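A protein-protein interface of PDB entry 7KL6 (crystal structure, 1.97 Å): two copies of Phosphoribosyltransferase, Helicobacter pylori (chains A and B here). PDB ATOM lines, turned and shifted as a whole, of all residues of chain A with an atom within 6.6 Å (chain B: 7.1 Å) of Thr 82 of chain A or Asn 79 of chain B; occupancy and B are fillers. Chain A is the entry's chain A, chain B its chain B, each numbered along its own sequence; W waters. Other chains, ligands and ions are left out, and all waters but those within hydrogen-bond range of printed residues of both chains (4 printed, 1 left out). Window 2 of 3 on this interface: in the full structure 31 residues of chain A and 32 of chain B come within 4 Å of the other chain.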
ATOM      1  N   GLU A  57      22.731  26.426 -21.162  1.00  0.00           N
ATOM      2  CA  GLU A  57      21.470  27.107 -20.857  1.00  0.00           C
ATOM      3  C   GLU A  57      20.328  26.257 -21.387  1.00  0.00           C
ATOM      4  O   GLU A  57      19.910  26.375 -22.544  1.00  0.00           O
ATOM      5  CB  GLU A  57      21.464  28.506 -21.453  1.00  0.00           C
ATOM      6  CG  GLU A  57      22.413  29.449 -20.739  1.00  0.00           C
ATOM      7  CD  GLU A  57      21.929  29.788 -19.335  1.00  0.00           C
ATOM      8  OE1 GLU A  57      20.696  29.735 -19.077  1.00  0.00           O
ATOM      9  OE2 GLU A  57      22.776  30.116 -18.491  1.00  0.00           O
ATOM     10  N   VAL A  58      19.834  25.364 -20.539  1.00  0.00           N
ATOM     11  CA  VAL A  58      18.749  24.455 -20.891  1.00  0.00           C
ATOM     12  C   VAL A  58      17.631  24.678 -19.879  1.00  0.00           C
ATOM     13  O   VAL A  58      17.882  24.671 -18.668  1.00  0.00           O
ATOM     14  CB  VAL A  58      19.235  22.994 -20.904  1.00  0.00           C
ATOM     15  CG1 VAL A  58      18.079  22.030 -21.166  1.00  0.00           C
ATOM     16  CG2 VAL A  58      20.342  22.825 -21.949  1.00  0.00           C
ATOM     17  N   TYR A  59      16.419  24.944 -20.382  1.00  0.00           N
ATOM     18  CA  TYR A  59      15.255  25.277 -19.576  1.00  0.00           C
ATOM     19  C   TYR A  59      14.189  24.224 -19.837  1.00  0.00           C
ATOM     20  O   TYR A  59      14.197  23.571 -20.882  1.00  0.00           O
ATOM     21  CB  TYR A  59      14.690  26.676 -19.920  1.00  0.00           C
ATOM     22  CG  TYR A  59      15.670  27.818 -19.696  1.00  0.00           C
ATOM     23  CD1 TYR A  59      16.622  28.157 -20.669  1.00  0.00           C
ATOM     24  CD2 TYR A  59      15.644  28.556 -18.517  1.00  0.00           C
ATOM     25  CE1 TYR A  59      17.526  29.188 -20.471  1.00  0.00           C
ATOM     26  CE2 TYR A  59      16.548  29.609 -18.309  1.00  0.00           C
ATOM     27  CZ  TYR A  59      17.483  29.917 -19.286  1.00  0.00           C
ATOM     28  OH  TYR A  59      18.370  30.956 -19.089  1.00  0.00           O
ATOM     29  N   ASN A  79       5.123  25.749 -15.185  1.00  0.00           N
ATOM     30  CA  ASN A  79       6.564  25.823 -14.932  1.00  0.00           C
ATOM     31  C   ASN A  79       7.265  26.640 -16.020  1.00  0.00           C
ATOM     32  O   ASN A  79       8.266  26.226 -16.610  1.00  0.00           O
ATOM     33  CB  ASN A  79       7.170  24.418 -14.803  1.00  0.00           C
ATOM     34  CG  ASN A  79       6.413  23.548 -13.799  1.00  0.00           C
ATOM     35  OD1 ASN A  79       5.966  24.031 -12.765  1.00  0.00           O
ATOM     36  ND2 ASN A  79       6.266  22.264 -14.107  1.00  0.00           N
ATOM     37  N   ILE A  80       6.697  27.803 -16.310  1.00  0.00           N
ATOM     38  CA  ILE A  80       7.223  28.696 -17.334  1.00  0.00           C
ATOM     39  C   ILE A  80       8.602  29.211 -16.943  1.00  0.00           C
ATOM     40  O   ILE A  80       8.760  29.839 -15.888  1.00  0.00           O
ATOM     41  CB  ILE A  80       6.235  29.840 -17.597  1.00  0.00           C
ATOM     42  CG1 ILE A  80       4.812  29.254 -17.689  1.00  0.00           C
ATOM     43  CG2 ILE A  80       6.688  30.692 -18.799  1.00  0.00           C
ATOM     44  CD1 ILE A  80       3.716  30.281 -17.763  1.00  0.00           C
ATOM     45  N   PRO A  81       9.618  28.965 -17.758  1.00  0.00           N
ATOM     46  CA  PRO A  81      10.977  29.361 -17.381  1.00  0.00           C
ATOM     47  C   PRO A  81      11.161  30.867 -17.487  1.00  0.00           C
ATOM     48  O   PRO A  81      10.454  31.549 -18.230  1.00  0.00           O
ATOM     49  CB  PRO A  81      11.854  28.626 -18.399  1.00  0.00           C
ATOM     50  CG  PRO A  81      10.966  28.476 -19.614  1.00  0.00           C
ATOM     51  CD  PRO A  81       9.565  28.284 -19.065  1.00  0.00           C
ATOM     52  N   THR A  82      12.118  31.381 -16.717  1.00  0.00           N
ATOM     53  CA  THR A  82      12.595  32.756 -16.857  1.00  0.00           C
ATOM     54  C   THR A  82      13.966  32.679 -17.517  1.00  0.00           C
ATOM     55  O   THR A  82      14.964  32.335 -16.876  1.00  0.00           O
ATOM     56  CB  THR A  82      12.656  33.487 -15.516  1.00  0.00           C
ATOM     57  OG1 THR A  82      11.419  33.309 -14.820  1.00  0.00           O
ATOM     58  CG2 THR A  82      12.865  34.989 -15.737  1.00  0.00           C
ATOM     59  N   ILE A  83      14.005  32.984 -18.805  1.00  0.00           N
ATOM     60  CA  ILE A  83      15.234  32.874 -19.571  1.00  0.00           C
ATOM     61  C   ILE A  83      16.060  34.132 -19.343  1.00  0.00           C
ATOM     62  O   ILE A  83      15.522  35.246 -19.305  1.00  0.00           O
ATOM     63  CB  ILE A  83      14.899  32.657 -21.061  1.00  0.00           C
ATOM     64  CG1 ILE A  83      14.097  31.364 -21.240  1.00  0.00           C
ATOM     65  CG2 ILE A  83      16.172  32.671 -21.920  1.00  0.00           C
ATOM     66  CD1 ILE A  83      13.443  31.245 -22.624  1.00  0.00           C
ATOM     67  N   LYS A  84      17.370  33.963 -19.177  1.00  0.00           N
ATOM     68  CA  LYS A  84      18.237  35.090 -18.853  1.00  0.00           C
ATOM     69  C   LYS A  84      18.272  36.108 -19.991  1.00  0.00           C
ATOM     70  O   LYS A  84      18.070  35.776 -21.164  1.00  0.00           O
ATOM     71  CB  LYS A  84      19.657  34.604 -18.562  1.00  0.00           C
ATOM     72  CG  LYS A  84      19.772  33.650 -17.379  1.00  0.00           C
ATOM     73  CD  LYS A  84      21.207  33.132 -17.288  1.00  0.00           C
ATOM     74  CE  LYS A  84      21.363  32.080 -16.206  1.00  0.00           C
ATOM     75  NZ  LYS A  84      22.751  31.531 -16.192  1.00  0.00           N
ATOM     76  N   LYS A 113       6.126  36.120 -22.468  1.00  0.00           N
ATOM     77  CA  LYS A 113       6.968  36.422 -21.317  1.00  0.00           C
ATOM     78  C   LYS A 113       8.324  37.001 -21.722  1.00  0.00           C
ATOM     79  O   LYS A 113       8.931  37.751 -20.949  1.00  0.00           O
ATOM     80  CB  LYS A 113       7.143  35.167 -20.478  1.00  0.00           C
ATOM     81  CG  LYS A 113       7.939  35.355 -19.206  1.00  0.00           C
ATOM     82  CD  LYS A 113       8.048  34.029 -18.470  1.00  0.00           C
ATOM     83  CE  LYS A 113       8.830  34.172 -17.189  1.00  0.00           C
ATOM     84  NZ  LYS A 113       8.838  32.899 -16.429  1.00  0.00           N
ATOM     85  N   HIS A 114       8.813  36.690 -22.917  1.00  0.00           N
ATOM     86  CA  HIS A 114      10.106  37.193 -23.377  1.00  0.00           C
ATOM     87  C   HIS A 114       9.938  37.842 -24.748  1.00  0.00           C
ATOM     88  O   HIS A 114      10.382  37.292 -25.767  1.00  0.00           O
ATOM     89  CB  HIS A 114      11.134  36.064 -23.433  1.00  0.00           C
ATOM     90  CG  HIS A 114      11.186  35.193 -22.209  1.00  0.00           C
ATOM     91  ND1 HIS A 114      10.363  34.097 -22.040  1.00  0.00           N
ATOM     92  CD2 HIS A 114      12.028  35.195 -21.146  1.00  0.00           C
ATOM     93  CE1 HIS A 114      10.676  33.480 -20.911  1.00  0.00           C
ATOM     94  NE2 HIS A 114      11.681  34.126 -20.347  1.00  0.00           N
ATOM     95  N   LYS A 117      13.005  38.075 -27.332  1.00  0.00           N
ATOM     96  CA  LYS A 117      13.787  36.943 -27.802  1.00  0.00           C
ATOM     97  C   LYS A 117      13.155  36.340 -29.049  1.00  0.00           C
ATOM     98  O   LYS A 117      11.982  36.561 -29.343  1.00  0.00           O
ATOM     99  CB  LYS A 117      13.904  35.902 -26.695  1.00  0.00           C
ATOM    100  CG  LYS A 117      14.422  36.493 -25.370  1.00  0.00           C
ATOM    101  CD  LYS A 117      14.623  35.398 -24.321  1.00  0.00           C
ATOM    102  CE  LYS A 117      15.059  36.029 -22.987  1.00  0.00           C
ATOM    103  NZ  LYS A 117      16.214  36.957 -23.130  1.00  0.00           N
ATOM    104  N   MET B  39      19.470  19.354 -14.447  1.00  0.00           N
ATOM    105  CA  MET B  39      19.910  19.558 -15.825  1.00  0.00           C
ATOM    106  C   MET B  39      21.386  19.942 -15.854  1.00  0.00           C
ATOM    107  O   MET B  39      21.858  20.642 -14.956  1.00  0.00           O
ATOM    108  CB  MET B  39      19.036  20.635 -16.469  1.00  0.00           C
ATOM    109  CG  MET B  39      17.546  20.324 -16.303  1.00  0.00           C
ATOM    110  SD  MET B  39      16.571  21.040 -17.605  1.00  0.00           S
ATOM    111  CE  MET B  39      14.964  20.341 -17.235  1.00  0.00           C
ATOM    112  N   TYR B  59       9.937  18.362 -13.059  1.00  0.00           N
ATOM    113  CA  TYR B  59      10.490  19.698 -12.903  1.00  0.00           C
ATOM    114  C   TYR B  59      11.972  19.673 -13.252  1.00  0.00           C
ATOM    115  O   TYR B  59      12.622  18.631 -13.187  1.00  0.00           O
ATOM    116  CB  TYR B  59      10.313  20.199 -11.463  1.00  0.00           C
ATOM    117  CG  TYR B  59       8.884  20.286 -10.980  1.00  0.00           C
ATOM    118  CD1 TYR B  59       8.245  19.187 -10.431  1.00  0.00           C
ATOM    119  CD2 TYR B  59       8.171  21.481 -11.067  1.00  0.00           C
ATOM    120  CE1 TYR B  59       6.924  19.267  -9.988  1.00  0.00           C
ATOM    121  CE2 TYR B  59       6.855  21.575 -10.621  1.00  0.00           C
ATOM    122  CZ  TYR B  59       6.239  20.467 -10.082  1.00  0.00           C
ATOM    123  OH  TYR B  59       4.933  20.567  -9.636  1.00  0.00           O
ATOM    124  N   GLY B  60      12.507  20.832 -13.635  1.00  0.00           N
ATOM    125  CA  GLY B  60      13.936  20.944 -13.886  1.00  0.00           C
ATOM    126  C   GLY B  60      14.625  21.883 -12.909  1.00  0.00           C
ATOM    127  O   GLY B  60      13.963  22.708 -12.267  1.00  0.00           O
ATOM    128  N   ILE B  61      15.941  21.736 -12.754  1.00  0.00           N
ATOM    129  CA  ILE B  61      16.743  22.653 -11.952  1.00  0.00           C
ATOM    130  C   ILE B  61      18.175  22.603 -12.477  1.00  0.00           C
ATOM    131  O   ILE B  61      18.655  21.548 -12.895  1.00  0.00           O
ATOM    132  CB  ILE B  61      16.675  22.307 -10.447  1.00  0.00           C
ATOM    133  CG1 ILE B  61      17.154  23.491  -9.581  1.00  0.00           C
ATOM    134  CG2 ILE B  61      17.502  21.042 -10.136  1.00  0.00           C
ATOM    135  CD1 ILE B  61      16.767  23.353  -8.104  1.00  0.00           C
ATOM    136  N   ASN B  62      18.847  23.752 -12.467  1.00  0.00           N
ATOM    137  CA  ASN B  62      20.218  23.893 -12.950  1.00  0.00           C
ATOM    138  C   ASN B  62      21.135  24.335 -11.814  1.00  0.00           C
ATOM    139  O   ASN B  62      20.715  25.046 -10.891  1.00  0.00           O
ATOM    140  CB  ASN B  62      20.343  24.950 -14.087  1.00  0.00           C
ATOM    141  CG  ASN B  62      19.372  24.733 -15.237  1.00  0.00           C
ATOM    142  OD1 ASN B  62      18.177  25.019 -15.115  1.00  0.00           O
ATOM    143  ND2 ASN B  62      19.892  24.272 -16.389  1.00  0.00           N
ATOM    144  N   ALA B  63      22.406  23.949 -11.911  1.00  0.00           N
ATOM    145  CA  ALA B  63      23.461  24.468 -11.050  1.00  0.00           C
ATOM    146  C   ALA B  63      24.638  24.937 -11.898  1.00  0.00           C
ATOM    147  O   ALA B  63      24.859  24.435 -13.003  1.00  0.00           O
ATOM    148  CB  ALA B  63      23.954  23.415 -10.047  1.00  0.00           C
ATOM    149  N   ILE B  77      22.273  27.803  -7.521  1.00  0.00           N
ATOM    150  CA  ILE B  77      21.258  26.926  -8.077  1.00  0.00           C
ATOM    151  C   ILE B  77      20.243  27.766  -8.823  1.00  0.00           C
ATOM    152  O   ILE B  77      19.742  28.788  -8.296  1.00  0.00           O
ATOM    153  CB  ILE B  77      20.583  26.087  -6.986  1.00  0.00           C
ATOM    154  CG1 ILE B  77      21.637  25.309  -6.198  1.00  0.00           C
ATOM    155  CG2 ILE B  77      19.634  25.142  -7.628  1.00  0.00           C
ATOM    156  CD1 ILE B  77      22.629  24.618  -7.101  1.00  0.00           C
ATOM    157  N   GLU B  78      19.926  27.329 -10.042  1.00  0.00           N
ATOM    158  CA  GLU B  78      19.217  28.206 -10.949  1.00  0.00           C
ATOM    159  C   GLU B  78      17.880  27.581 -11.323  1.00  0.00           C
ATOM    160  O   GLU B  78      17.689  26.362 -11.221  1.00  0.00           O
ATOM    161  CB  GLU B  78      19.907  28.322 -12.257  1.00  0.00           C
ATOM    162  CG  GLU B  78      21.341  28.733 -12.431  1.00  0.00           C
ATOM    163  CD  GLU B  78      21.691  30.074 -11.871  1.00  0.00           C
ATOM    164  OE1 GLU B  78      20.936  30.817 -11.149  1.00  0.00           O
ATOM    165  OE2 GLU B  78      22.505  30.577 -12.686  1.00  0.00           O
ATOM    166  N   ASN B  79      16.923  28.424 -11.717  1.00  0.00           N
ATOM    167  CA  ASN B  79      15.657  27.929 -12.255  1.00  0.00           C
ATOM    168  C   ASN B  79      14.963  27.012 -11.245  1.00  0.00           C
ATOM    169  O   ASN B  79      14.607  25.870 -11.553  1.00  0.00           O
ATOM    170  CB  ASN B  79      15.896  27.204 -13.590  1.00  0.00           C
ATOM    171  CG  ASN B  79      16.573  28.094 -14.654  1.00  0.00           C
ATOM    172  OD1 ASN B  79      16.139  29.215 -14.909  1.00  0.00           O
ATOM    173  ND2 ASN B  79      17.640  27.591 -15.259  1.00  0.00           N
ATOM    174  N   ILE B  80      14.770  27.516 -10.026  1.00  0.00           N
ATOM    175  CA  ILE B  80      14.271  26.672  -8.935  1.00  0.00           C
ATOM    176  C   ILE B  80      12.778  26.427  -9.102  1.00  0.00           C
ATOM    177  O   ILE B  80      11.995  27.381  -9.077  1.00  0.00           O
ATOM    178  CB  ILE B  80      14.563  27.295  -7.565  1.00  0.00           C
ATOM    179  CG1 ILE B  80      16.067  27.555  -7.415  1.00  0.00           C
ATOM    180  CG2 ILE B  80      14.021  26.385  -6.466  1.00  0.00           C
ATOM    181  CD1 ILE B  80      16.386  28.699  -6.486  1.00  0.00           C
ATOM    182  N   PRO B  81      12.333  25.182  -9.241  1.00  0.00           N
ATOM    183  CA  PRO B  81      10.913  24.938  -9.497  1.00  0.00           C
ATOM    184  C   PRO B  81      10.053  25.287  -8.295  1.00  0.00           C
ATOM    185  O   PRO B  81      10.517  25.350  -7.155  1.00  0.00           O
ATOM    186  CB  PRO B  81      10.859  23.438  -9.795  1.00  0.00           C
ATOM    187  CG  PRO B  81      12.043  22.881  -9.123  1.00  0.00           C
ATOM    188  CD  PRO B  81      13.105  23.929  -9.182  1.00  0.00           C
ATOM    189  N   THR B  82       8.771  25.514  -8.572  1.00  0.00           N
ATOM    190  CA  THR B  82       7.749  25.668  -7.544  1.00  0.00           C
ATOM    191  C   THR B  82       6.834  24.452  -7.648  1.00  0.00           C
ATOM    192  O   THR B  82       5.994  24.367  -8.549  1.00  0.00           O
ATOM    193  CB  THR B  82       6.990  26.978  -7.708  1.00  0.00           C
ATOM    194  OG1 THR B  82       7.909  28.066  -7.592  1.00  0.00           O
ATOM    195  CG2 THR B  82       5.935  27.112  -6.633  1.00  0.00           C
ATOM    196  N   LYS B 113      12.703  25.656   0.188  1.00  0.00           N
ATOM    197  CA  LYS B 113      11.545  26.267  -0.444  1.00  0.00           C
ATOM    198  C   LYS B 113      10.274  25.475  -0.158  1.00  0.00           C
ATOM    199  O   LYS B 113       9.187  26.058  -0.083  1.00  0.00           O
ATOM    200  CB  LYS B 113      11.810  26.396  -1.944  1.00  0.00           C
ATOM    201  CG  LYS B 113      10.667  26.953  -2.747  1.00  0.00           C
ATOM    202  CD  LYS B 113      11.087  27.184  -4.190  1.00  0.00           C
ATOM    203  CE  LYS B 113       9.913  27.714  -4.984  1.00  0.00           C
ATOM    204  NZ  LYS B 113      10.298  28.017  -6.383  1.00  0.00           N
HETATM  205  O   HOH W   1       3.895  23.027 -11.415  1.00  0.00           O
HETATM  206  O   HOH W   2      13.589  29.326 -14.991  1.00  0.00           O
HETATM  207  O   HOH W   3      20.063  28.967 -16.101  1.00  0.00           O
HETATM  208  O   HOH W   4       8.030  25.654 -11.357  1.00  0.00           O
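The side-chain amide nitrogen (ND2) of Asn 62 of chain B lies within hydrogen-bond range of the backbone carbonyl oxygen (O) of Val 58 of chain A (3.1 Å). The side-chain carboxylate of Glu 78 of chain B is in salt-bridge range of the side-chain amino group of Lys 84 of chain A, at 3.6 Å.
OH of Tyr 59 of chain A lies within hydrogen-bond range of OE1 of Glu 57 of chain A. N of Lys 84 of chain A lies within hydrogen-bond range of OH of Tyr 59 of chain A (3.2 Å). The side-chain hydroxyl of Thr 82 of chain A is in hydrogen-bond range of the side-chain amino group of Lys 113 of chain A, at 3.1 Å. The backbone carbonyl oxygen (O) of Lys 84 of chain A lies within hydrogen-bond range of the side-chain amino group (NZ) of Lys 117 of chain A (3.0 Å). The backbone NH (N) of Met 39 of chain B is in hydrogen-bond range of the backbone carbonyl oxygen (O) of Ile 61 of chain B (2.8 Å). O of Asn 62 of chain B lies within hydrogen-bond range of N of Glu 78 of chain B, 2.6 Å away.
Val 58 of chain A touches Met 39 of chain B (CG1 to SD, 3.99 Å). Tyr 59 of chain A touches Asn 79 of chain B (CE2 to OD1, 3.4 Å). Asn 79 of chain A touches Tyr 59 of chain B (OD1 to CE2, 3.4 Å). OD1 of Asn 79 of chain B touches O of Thr 82 of chain A, 3.9 Å away.
Of the printed residues of chain B, Val 58 of chain A touches Met 39 and Asn 62. Printed residues of chain B within 4 Å of Tyr 59 of chain A: Asn 79 (3.4 Å). Of the printed residues of chain B, Asn 79 of chain A touches Tyr 59 (3.4 Å). Thr 82 of chain A touches one residue of chain B. Of the printed residues of chain A, Met 39 of chain B touches Val 58. Printed residues of chain A within 4 Å of Asn 62 of chain B: Val 58. Of chain A, only Tyr 59 (3.4 Å) and Thr 82 (3.9 Å) come within 4 Å of Asn 79 of chain B. The nearest residue of chain A that does not touch Asn 79 of chain B is Val 58 of chain A (4.5 Å). The nearest printed residue of chain A that does not touch Tyr 59 of chain B is Tyr 59 of chain A (8.3 Å).
Of the 13 printed residues of chain B, 5 touch a printed residue of chain A. Printed residues of chain B that touch a printed residue of chain A: Met 39, Tyr 59, Asn 62, Glu 78 and Asn 79. Along chain B the printed residues that touch a printed residue of chain A span positions 39 to 79. Of the 12 printed residues of chain A, 5 touch a printed residue of chain B. Hydrophobic or aromatic side chains of chain A that line the printed part of chain B: Val 58 and Tyr 59. Among the printed residues, Asp or Glu carboxylates within 4 Å of a Lys or Arg side-chain nitrogen of the other chain: Lys 84 of chain A with Glu 78 of chain B (3.6 Å).
Tyr 59 of chain A touches Asn 79 of chain B, and with the chains exchanged Asn 79 of chain A touches Tyr 59 of chain B. Thr 82 of chain A touches Asn 79 of chain B, but with the chains exchanged Asn 79 of chain A does not touch Thr 82 of chain B (4.2 Å). Positions printed for both chains: 59, 79, 80, 81, 82 and 113. Of the 6 pairs that touch across the chains among the printed residues, 2 have their exchanged pair printed and touching as well.
Water W2 lies within hydrogen-bond range of the side-chain amide oxygen (OD1) of Asn 79 of chain B and the backbone NH (N) of Thr 82 of chain A. Water W1 bridges OD1 of Asn 79 of chain A (2.7 Å) and OH of Tyr 59 of chain B (3.2 Å). Water W4 bridges N of Thr 82 of chain B and OD1 of Asn 79 of chain A. Water W3 lies within hydrogen-bond range of ND2 of Asn 79 of chain B (2.9 Å) and OE1 of Glu 57 of chain A (3.1 Å).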
